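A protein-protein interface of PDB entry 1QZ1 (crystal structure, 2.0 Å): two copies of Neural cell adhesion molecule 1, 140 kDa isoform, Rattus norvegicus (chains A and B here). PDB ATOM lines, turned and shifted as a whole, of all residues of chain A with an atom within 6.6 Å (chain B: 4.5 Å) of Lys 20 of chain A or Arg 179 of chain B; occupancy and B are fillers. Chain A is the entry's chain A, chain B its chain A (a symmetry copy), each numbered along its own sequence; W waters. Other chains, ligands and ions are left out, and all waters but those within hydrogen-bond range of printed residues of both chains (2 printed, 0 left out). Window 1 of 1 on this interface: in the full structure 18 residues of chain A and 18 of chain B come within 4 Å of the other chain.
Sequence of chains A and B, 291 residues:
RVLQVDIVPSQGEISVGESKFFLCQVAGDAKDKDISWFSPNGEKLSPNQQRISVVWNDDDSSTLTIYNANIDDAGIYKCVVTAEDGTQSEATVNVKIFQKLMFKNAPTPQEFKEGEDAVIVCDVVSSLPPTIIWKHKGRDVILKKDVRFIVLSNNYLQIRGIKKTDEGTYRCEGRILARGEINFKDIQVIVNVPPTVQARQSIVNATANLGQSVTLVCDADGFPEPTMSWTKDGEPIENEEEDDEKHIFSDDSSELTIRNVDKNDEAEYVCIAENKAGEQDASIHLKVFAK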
ATOM      1  N   VAL A   8      -2.136  11.547  -0.840  1.00  0.00           N
ATOM      2  CA  VAL A   8      -0.702  11.776  -0.704  1.00  0.00           C
ATOM      3  C   VAL A   8      -0.096  11.954  -2.093  1.00  0.00           C
ATOM      4  O   VAL A   8      -0.340  11.146  -2.994  1.00  0.00           O
ATOM      5  CB  VAL A   8      -0.006  10.593  -0.023  1.00  0.00           C
ATOM      6  CG1 VAL A   8       1.492  10.832   0.026  1.00  0.00           C
ATOM      7  CG2 VAL A   8      -0.554  10.416   1.375  1.00  0.00           C
ATOM      8  N   PRO A   9       0.647  13.049  -2.303  1.00  0.00           N
ATOM      9  CA  PRO A   9       0.956  14.129  -1.353  1.00  0.00           C
ATOM     10  C   PRO A   9      -0.309  14.937  -1.058  1.00  0.00           C
ATOM     11  O   PRO A   9      -1.199  15.048  -1.906  1.00  0.00           O
ATOM     12  CB  PRO A   9       2.026  14.940  -2.087  1.00  0.00           C
ATOM     13  CG  PRO A   9       1.709  14.686  -3.545  1.00  0.00           C
ATOM     14  CD  PRO A   9       1.424  13.208  -3.543  1.00  0.00           C
ATOM     15  N   GLN A  11      -0.805  17.979  -0.940  1.00  0.00           N
ATOM     16  CA  GLN A  11      -0.970  19.151  -1.788  1.00  0.00           C
ATOM     17  C   GLN A  11       0.081  19.101  -2.883  1.00  0.00           C
ATOM     18  O   GLN A  11       1.075  18.381  -2.768  1.00  0.00           O
ATOM     19  CB  GLN A  11      -0.864  20.443  -0.971  1.00  0.00           C
ATOM     20  CG  GLN A  11       0.396  20.575  -0.106  1.00  0.00           C
ATOM     21  CD  GLN A  11       0.409  21.883   0.691  1.00  0.00           C
ATOM     22  OE1 GLN A  11       0.307  22.966   0.114  1.00  0.00           O
ATOM     23  NE2 GLN A  11       0.532  21.787   2.018  1.00  0.00           N
ATOM     24  N   GLY A  12      -0.142  19.828  -3.970  1.00  0.00           N
ATOM     25  CA  GLY A  12       0.837  19.775  -5.039  1.00  0.00           C
ATOM     26  C   GLY A  12       0.928  20.998  -5.923  1.00  0.00           C
ATOM     27  O   GLY A  12      -0.009  21.782  -6.048  1.00  0.00           O
ATOM     28  N   GLU A  13       2.091  21.158  -6.536  1.00  0.00           N
ATOM     29  CA  GLU A  13       2.318  22.268  -7.445  1.00  0.00           C
ATOM     30  C   GLU A  13       2.964  21.661  -8.687  1.00  0.00           C
ATOM     31  O   GLU A  13       3.861  20.831  -8.570  1.00  0.00           O
ATOM     32  CB  GLU A  13       3.249  23.302  -6.799  1.00  0.00           C
ATOM     33  CG  GLU A  13       3.464  24.532  -7.652  1.00  0.00           C
ATOM     34  CD  GLU A  13       4.229  25.624  -6.923  1.00  0.00           C
ATOM     35  OE1 GLU A  13       5.409  25.401  -6.573  1.00  0.00           O
ATOM     36  OE2 GLU A  13       3.637  26.702  -6.695  1.00  0.00           O
ATOM     37  N   ILE A  14       2.505  22.050  -9.872  1.00  0.00           N
ATOM     38  CA  ILE A  14       3.068  21.489 -11.098  1.00  0.00           C
ATOM     39  C   ILE A  14       3.408  22.581 -12.092  1.00  0.00           C
ATOM     40  O   ILE A  14       2.582  23.455 -12.370  1.00  0.00           O
ATOM     41  CB  ILE A  14       2.085  20.545 -11.804  1.00  0.00           C
ATOM     42  CG1 ILE A  14       1.371  19.666 -10.775  1.00  0.00           C
ATOM     43  CG2 ILE A  14       2.843  19.667 -12.816  1.00  0.00           C
ATOM     44  CD1 ILE A  14       0.226  18.877 -11.368  1.00  0.00           C
ATOM     45  N   GLU A  18       4.786  19.767 -17.076  1.00  0.00           N
ATOM     46  CA  GLU A  18       5.271  18.635 -16.288  1.00  0.00           C
ATOM     47  C   GLU A  18       4.144  17.761 -15.749  1.00  0.00           C
ATOM     48  O   GLU A  18       2.970  18.013 -16.016  1.00  0.00           O
ATOM     49  CB  GLU A  18       6.200  19.133 -15.172  1.00  0.00           C
ATOM     50  CG  GLU A  18       7.408  19.861 -15.765  1.00  0.00           C
ATOM     51  CD  GLU A  18       8.404  20.361 -14.737  1.00  0.00           C
ATOM     52  OE1 GLU A  18       8.244  20.061 -13.536  1.00  0.00           O
ATOM     53  OE2 GLU A  18       9.360  21.058 -15.144  1.00  0.00           O
ATOM     54  N   SER A  19       4.504  16.718 -15.013  1.00  0.00           N
ATOM     55  CA  SER A  19       3.511  15.789 -14.501  1.00  0.00           C
ATOM     56  C   SER A  19       3.631  15.531 -13.001  1.00  0.00           C
ATOM     57  O   SER A  19       4.697  15.712 -12.424  1.00  0.00           O
ATOM     58  CB  SER A  19       3.624  14.469 -15.274  1.00  0.00           C
ATOM     59  OG  SER A  19       3.455  14.682 -16.671  1.00  0.00           O
ATOM     60  N   LYS A  20       2.524  15.131 -12.372  1.00  0.00           N
ATOM     61  CA  LYS A  20       2.485  14.829 -10.939  1.00  0.00           C
ATOM     62  C   LYS A  20       1.352  13.863 -10.695  1.00  0.00           C
ATOM     63  O   LYS A  20       0.408  13.786 -11.481  1.00  0.00           O
ATOM     64  CB  LYS A  20       2.233  16.082 -10.096  1.00  0.00           C
ATOM     65  CG  LYS A  20       3.482  16.747  -9.560  1.00  0.00           C
ATOM     66  CD  LYS A  20       3.365  16.960  -8.064  1.00  0.00           C
ATOM     67  CE  LYS A  20       4.535  17.766  -7.518  1.00  0.00           C
ATOM     68  NZ  LYS A  20       5.859  17.153  -7.832  1.00  0.00           N
ATOM     69  N   PHE A  21       1.428  13.127  -9.605  1.00  0.00           N
ATOM     70  CA  PHE A  21       0.367  12.193  -9.323  1.00  0.00           C
ATOM     71  C   PHE A  21      -0.003  12.288  -7.866  1.00  0.00           C
ATOM     72  O   PHE A  21       0.769  12.801  -7.045  1.00  0.00           O
ATOM     73  CB  PHE A  21       0.783  10.773  -9.713  1.00  0.00           C
ATOM     74  CG  PHE A  21       1.814  10.158  -8.820  1.00  0.00           C
ATOM     75  CD1 PHE A  21       1.432   9.348  -7.754  1.00  0.00           C
ATOM     76  CD2 PHE A  21       3.178  10.339  -9.073  1.00  0.00           C
ATOM     77  CE1 PHE A  21       2.399   8.700  -6.966  1.00  0.00           C
ATOM     78  CE2 PHE A  21       4.137   9.703  -8.297  1.00  0.00           C
ATOM     79  CZ  PHE A  21       3.749   8.884  -7.237  1.00  0.00           C
ATOM     80  N   PHE A  22      -1.193  11.784  -7.554  1.00  0.00           N
ATOM     81  CA  PHE A  22      -1.727  11.832  -6.213  1.00  0.00           C
ATOM     82  C   PHE A  22      -2.450  10.531  -5.918  1.00  0.00           C
ATOM     83  O   PHE A  22      -3.264  10.064  -6.717  1.00  0.00           O
ATOM     84  CB  PHE A  22      -2.701  13.015  -6.101  1.00  0.00           C
ATOM     85  CG  PHE A  22      -2.103  14.317  -6.524  1.00  0.00           C
ATOM     86  CD1 PHE A  22      -2.117  14.705  -7.863  1.00  0.00           C
ATOM     87  CD2 PHE A  22      -1.470  15.137  -5.593  1.00  0.00           C
ATOM     88  CE1 PHE A  22      -1.504  15.893  -8.269  1.00  0.00           C
ATOM     89  CE2 PHE A  22      -0.851  16.331  -5.991  1.00  0.00           C
ATOM     90  CZ  PHE A  22      -0.870  16.706  -7.331  1.00  0.00           C
ATOM     91  N   LEU A  64      -4.495   9.455  -9.163  1.00  0.00           N
ATOM     92  CA  LEU A  64      -4.785  10.476 -10.148  1.00  0.00           C
ATOM     93  C   LEU A  64      -3.446  10.980 -10.671  1.00  0.00           C
ATOM     94  O   LEU A  64      -2.605  11.433  -9.888  1.00  0.00           O
ATOM     95  CB  LEU A  64      -5.550  11.638  -9.508  1.00  0.00           C
ATOM     96  CG  LEU A  64      -5.552  12.919 -10.347  1.00  0.00           C
ATOM     97  CD1 LEU A  64      -6.300  12.676 -11.634  1.00  0.00           C
ATOM     98  CD2 LEU A  64      -6.181  14.065  -9.581  1.00  0.00           C
ATOM     99  N   THR A  65      -3.216  10.877 -11.975  1.00  0.00           N
ATOM    100  CA  THR A  65      -1.970  11.391 -12.539  1.00  0.00           C
ATOM    101  C   THR A  65      -2.300  12.508 -13.506  1.00  0.00           C
ATOM    102  O   THR A  65      -3.130  12.340 -14.393  1.00  0.00           O
ATOM    103  CB  THR A  65      -1.169  10.330 -13.337  1.00  0.00           C
ATOM    104  OG1 THR A  65      -0.876   9.209 -12.501  1.00  0.00           O
ATOM    105  CG2 THR A  65       0.138  10.932 -13.847  1.00  0.00           C
ATOM    106  N   ILE A  66      -1.657  13.650 -13.340  1.00  0.00           N
ATOM    107  CA  ILE A  66      -1.891  14.767 -14.243  1.00  0.00           C
ATOM    108  C   ILE A  66      -0.639  14.907 -15.098  1.00  0.00           C
ATOM    109  O   ILE A  66       0.385  15.400 -14.626  1.00  0.00           O
ATOM    110  CB  ILE A  66      -2.147  16.087 -13.475  1.00  0.00           C
ATOM    111  CG1 ILE A  66      -3.459  15.978 -12.690  1.00  0.00           C
ATOM    112  CG2 ILE A  66      -2.198  17.269 -14.453  1.00  0.00           C
ATOM    113  CD1 ILE A  66      -3.819  17.213 -11.895  1.00  0.00           C
ATOM    114  N   TYR A  67      -0.731  14.447 -16.346  1.00  0.00           N
ATOM    115  CA  TYR A  67       0.378  14.513 -17.293  1.00  0.00           C
ATOM    116  C   TYR A  67       0.346  15.809 -18.069  1.00  0.00           C
ATOM    117  O   TYR A  67      -0.728  16.376 -18.282  1.00  0.00           O
ATOM    118  CB  TYR A  67       0.281  13.384 -18.318  1.00  0.00           C
ATOM    119  CG  TYR A  67       0.557  12.014 -17.778  1.00  0.00           C
ATOM    120  CD1 TYR A  67      -0.471  11.090 -17.603  1.00  0.00           C
ATOM    121  CD2 TYR A  67       1.862  11.631 -17.454  1.00  0.00           C
ATOM    122  CE1 TYR A  67      -0.212   9.811 -17.120  1.00  0.00           C
ATOM    123  CE2 TYR A  67       2.142  10.338 -16.970  1.00  0.00           C
ATOM    124  CZ  TYR A  67       1.095   9.441 -16.809  1.00  0.00           C
ATOM    125  OH  TYR A  67       1.359   8.177 -16.357  1.00  0.00           O
ATOM    126  N   ASN A  68       1.517  16.262 -18.506  1.00  0.00           N
ATOM    127  CA  ASN A  68       1.632  17.467 -19.318  1.00  0.00           C
ATOM    128  C   ASN A  68       0.697  18.583 -18.858  1.00  0.00           C
ATOM    129  O   ASN A  68      -0.144  19.058 -19.626  1.00  0.00           O
ATOM    130  CB  ASN A  68       1.311  17.109 -20.761  1.00  0.00           C
ATOM    131  CG  ASN A  68       1.574  18.257 -21.713  1.00  0.00           C
ATOM    132  OD1 ASN A  68       0.982  18.330 -22.789  1.00  0.00           O
ATOM    133  ND2 ASN A  68       2.472  19.158 -21.326  1.00  0.00           N
ATOM    134  N   ALA A  69       0.869  19.018 -17.616  1.00  0.00           N
ATOM    135  CA  ALA A  69       0.000  20.036 -17.036  1.00  0.00           C
ATOM    136  C   ALA A  69      -0.078  21.376 -17.731  1.00  0.00           C
ATOM    137  O   ALA A  69       0.909  21.884 -18.265  1.00  0.00           O
ATOM    138  CB  ALA A  69       0.369  20.263 -15.583  1.00  0.00           C
ATOM    139  N   VAL A  95      -4.368  21.628  -6.200  1.00  0.00           N
ATOM    140  CA  VAL A  95      -3.302  21.520  -7.172  1.00  0.00           C
ATOM    141  C   VAL A  95      -3.045  22.879  -7.797  1.00  0.00           C
ATOM    142  O   VAL A  95      -3.923  23.444  -8.449  1.00  0.00           O
ATOM    143  CB  VAL A  95      -3.656  20.498  -8.285  1.00  0.00           C
ATOM    144  CG1 VAL A  95      -2.512  20.398  -9.276  1.00  0.00           C
ATOM    145  CG2 VAL A  95      -3.929  19.123  -7.676  1.00  0.00           C
ATOM    146  N   GLU B  13      14.981  24.141  -0.356  1.00  0.00           N
ATOM    147  CA  GLU B  13      15.409  22.797  -0.701  1.00  0.00           C
ATOM    148  C   GLU B  13      16.117  22.920  -2.047  1.00  0.00           C
ATOM    149  O   GLU B  13      15.625  23.605  -2.940  1.00  0.00           O
ATOM    150  CB  GLU B  13      14.197  21.864  -0.808  1.00  0.00           C
ATOM    151  CG  GLU B  13      14.569  20.423  -1.078  1.00  0.00           C
ATOM    152  CD  GLU B  13      13.378  19.484  -0.992  1.00  0.00           C
ATOM    153  OE1 GLU B  13      12.444  19.619  -1.814  1.00  0.00           O
ATOM    154  OE2 GLU B  13      13.380  18.617  -0.091  1.00  0.00           O
ATOM    155  N   PHE B  98      18.761  17.536  -1.727  1.00  0.00           N
ATOM    156  CA  PHE B  98      18.206  16.253  -2.125  1.00  0.00           C
ATOM    157  C   PHE B  98      18.513  16.045  -3.593  1.00  0.00           C
ATOM    158  O   PHE B  98      19.092  16.912  -4.258  1.00  0.00           O
ATOM    159  CB  PHE B  98      16.695  16.185  -1.876  1.00  0.00           C
ATOM    160  CG  PHE B  98      15.873  16.892  -2.913  1.00  0.00           C
ATOM    161  CD1 PHE B  98      14.892  16.207  -3.629  1.00  0.00           C
ATOM    162  CD2 PHE B  98      16.077  18.242  -3.174  1.00  0.00           C
ATOM    163  CE1 PHE B  98      14.127  16.867  -4.594  1.00  0.00           C
ATOM    164  CE2 PHE B  98      15.324  18.912  -4.129  1.00  0.00           C
ATOM    165  CZ  PHE B  98      14.343  18.227  -4.845  1.00  0.00           C
ATOM    166  N   ILE B 176       7.891   8.890  -7.288  1.00  0.00           N
ATOM    167  CA  ILE B 176       8.245   8.992  -5.880  1.00  0.00           C
ATOM    168  C   ILE B 176       6.961   9.407  -5.188  1.00  0.00           C
ATOM    169  O   ILE B 176       6.569  10.570  -5.256  1.00  0.00           O
ATOM    170  CB  ILE B 176       9.327  10.043  -5.669  1.00  0.00           C
ATOM    171  CG1 ILE B 176      10.608   9.586  -6.369  1.00  0.00           C
ATOM    172  CG2 ILE B 176       9.568  10.241  -4.180  1.00  0.00           C
ATOM    173  CD1 ILE B 176      11.704  10.602  -6.369  1.00  0.00           C
ATOM    174  N   LEU B 177       6.308   8.466  -4.511  1.00  0.00           N
ATOM    175  CA  LEU B 177       5.019   8.757  -3.883  1.00  0.00           C
ATOM    176  C   LEU B 177       4.945   9.953  -2.950  1.00  0.00           C
ATOM    177  O   LEU B 177       4.028  10.767  -3.057  1.00  0.00           O
ATOM    178  CB  LEU B 177       4.474   7.538  -3.128  1.00  0.00           C
ATOM    179  CG  LEU B 177       3.171   7.860  -2.358  1.00  0.00           C
ATOM    180  CD1 LEU B 177       2.094   8.429  -3.322  1.00  0.00           C
ATOM    181  CD2 LEU B 177       2.661   6.611  -1.647  1.00  0.00           C
ATOM    182  N   ALA B 178       5.884  10.047  -2.015  1.00  0.00           N
ATOM    183  CA  ALA B 178       5.865  11.149  -1.065  1.00  0.00           C
ATOM    184  C   ALA B 178       5.797  12.510  -1.758  1.00  0.00           C
ATOM    185  O   ALA B 178       5.186  13.442  -1.235  1.00  0.00           O
ATOM    186  CB  ALA B 178       7.089  11.075  -0.145  1.00  0.00           C
ATOM    187  N   ARG B 179       6.401  12.630  -2.938  1.00  0.00           N
ATOM    188  CA  ARG B 179       6.389  13.901  -3.659  1.00  0.00           C
ATOM    189  C   ARG B 179       5.456  13.929  -4.863  1.00  0.00           C
ATOM    190  O   ARG B 179       5.312  14.966  -5.507  1.00  0.00           O
ATOM    191  CB  ARG B 179       7.801  14.244  -4.136  1.00  0.00           C
ATOM    192  CG  ARG B 179       8.805  14.389  -3.010  1.00  0.00           C
ATOM    193  CD  ARG B 179      10.182  14.791  -3.517  1.00  0.00           C
ATOM    194  NE  ARG B 179      11.006  15.215  -2.390  1.00  0.00           N
ATOM    195  CZ  ARG B 179      11.418  16.461  -2.187  1.00  0.00           C
ATOM    196  NH1 ARG B 179      11.100  17.422  -3.045  1.00  0.00           N
ATOM    197  NH2 ARG B 179      12.117  16.745  -1.099  1.00  0.00           N
ATOM    198  N   GLY B 180       4.833  12.794  -5.173  1.00  0.00           N
ATOM    199  CA  GLY B 180       3.955  12.735  -6.333  1.00  0.00           C
ATOM    200  C   GLY B 180       4.762  13.106  -7.565  1.00  0.00           C
ATOM    201  O   GLY B 180       4.245  13.623  -8.559  1.00  0.00           O
ATOM    202  N   GLU B 181       6.054  12.806  -7.495  1.00  0.00           N
ATOM    203  CA  GLU B 181       6.997  13.133  -8.555  1.00  0.00           C
ATOM    204  C   GLU B 181       7.032  12.086  -9.672  1.00  0.00           C
ATOM    205  O   GLU B 181       7.000  10.880  -9.418  1.00  0.00           O
ATOM    206  CB  GLU B 181       8.387  13.305  -7.915  1.00  0.00           C
ATOM    207  CG  GLU B 181       9.493  13.920  -8.759  1.00  0.00           C
ATOM    208  CD  GLU B 181      10.792  14.092  -7.941  1.00  0.00           C
ATOM    209  OE1 GLU B 181      10.915  13.452  -6.870  1.00  0.00           O
ATOM    210  OE2 GLU B 181      11.690  14.851  -8.368  1.00  0.00           O
ATOM    211  N   ILE B 182       7.112  12.572 -10.910  1.00  0.00           N
ATOM    212  CA  ILE B 182       7.160  11.718 -12.090  1.00  0.00           C
ATOM    213  C   ILE B 182       8.183  12.208 -13.074  1.00  0.00           C
ATOM    214  O   ILE B 182       8.302  13.407 -13.310  1.00  0.00           O
ATOM    215  CB  ILE B 182       5.828  11.707 -12.852  1.00  0.00           C
ATOM    216  CG1 ILE B 182       4.753  11.025 -12.022  1.00  0.00           C
ATOM    217  CG2 ILE B 182       5.996  10.998 -14.196  1.00  0.00           C
ATOM    218  CD1 ILE B 182       3.446  10.941 -12.753  1.00  0.00           C
HETATM  219  O   HOH W   1       6.958  15.418 -11.292  1.00  0.00           O
HETATM  220  O   HOH W   2       7.370  15.661 -14.824  1.00  0.00           O
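The backbone carbonyl oxygen (O) of Arg 179 of chain B is in hydrogen-bond range of the side-chain amino group (NZ) of Lys 20 of chain A (3.2 Å). The backbone carbonyl oxygen (O) of Gly 180 of chain B is in hydrogen-bond range of the backbone NH (N) of Phe 21 of chain A (3.0 Å).
The backbone carbonyl oxygen of Lys 20 of chain A sits at hydrogen-bond distance from the backbone NH of Ile 66 of chain A, 2.8 Å away. The side-chain carboxylate (OE2) of Glu 13 of chain B lies within salt-bridge range of the guanidinium group (NH2) of Arg 179 of chain B. N of Ile 176 of chain B lies within hydrogen-bond range of O of Glu 181 of chain B (3.0 Å).
Leu 177 of chain B touches Val 8 of chain A (CD1 to O, 3.7 Å). Pro 9 of chain A touches Leu 177 of chain B (CD to O, 3.6 Å). Pro 9 of chain A touches Ala 178 of chain B. Gly 180 of chain B touches Pro 9 of chain A (CA to CD, 3.8 Å). CA of Lys 20 of chain A touches O of Gly 180 of chain B, 3.2 Å away. CZ of Phe 21 of chain A touches O of Ile 176 of chain B, 3.8 Å away. CA of Leu 177 of chain B touches CZ of Phe 21 of chain A (3.6 Å). CE2 of Phe 21 of chain A touches O of Glu 181 of chain B (3.3 Å). Phe 21 of chain A touches Ile 182 of chain B (CD2 to CG1, 3.4 Å). Ile 182 of chain B touches Thr 65 of chain A.
Of the printed residues of chain B, Pro 9 of chain A touches Leu 177 (3.6 Å), Ala 178 (3.6 Å) and Gly 180 (3.8 Å). Lys 20 of chain A touches just these residues of chain B: Arg 179 (3.2 Å) and Gly 180 (3.2 Å). Printed residues of chain B within 4 Å of Phe 21 of chain A: Ile 176 (3.8 Å), Leu 177 (3.6 Å), Gly 180 (3.0 Å), Glu 181 (3.3 Å) and Ile 182 (3.4 Å). Phe 22 of chain A touches none of the printed residues of chain B. Of chain A, only Lys 20 (3.2 Å) comes within 4 Å of Arg 179 of chain B. Of the printed residues of chain A, Gly 180 of chain B touches Pro 9, Lys 20 and Phe 21. The nearest residue of chain A that does not touch Arg 179 of chain B is Pro 9 of chain A (4.04 Å).
Along chain B the printed residues that touch a printed residue of chain A span positions 176 to 182. Of the 18 printed residues of chain A, 5 touch a printed residue of chain B. Hydrophobic or aromatic side chains of chain A that line the printed part of chain B: Val 8, Pro 9 and Phe 21.
Position printed for both chains: 13. Of the 12 pairs that touch across the chains among the printed residues, none has its exchanged pair printed and touching as well.
Water W1 lies within hydrogen-bond range of the backbone carbonyl oxygen of Ser 19 of chain A (2.5 Å) and the backbone NH of Ile 182 of chain B (2.9 Å). Water W2 lies within hydrogen-bond range of the backbone carbonyl oxygen (O) of Ile 182 of chain B and the backbone NH (N) of Ser 19 of chain A.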
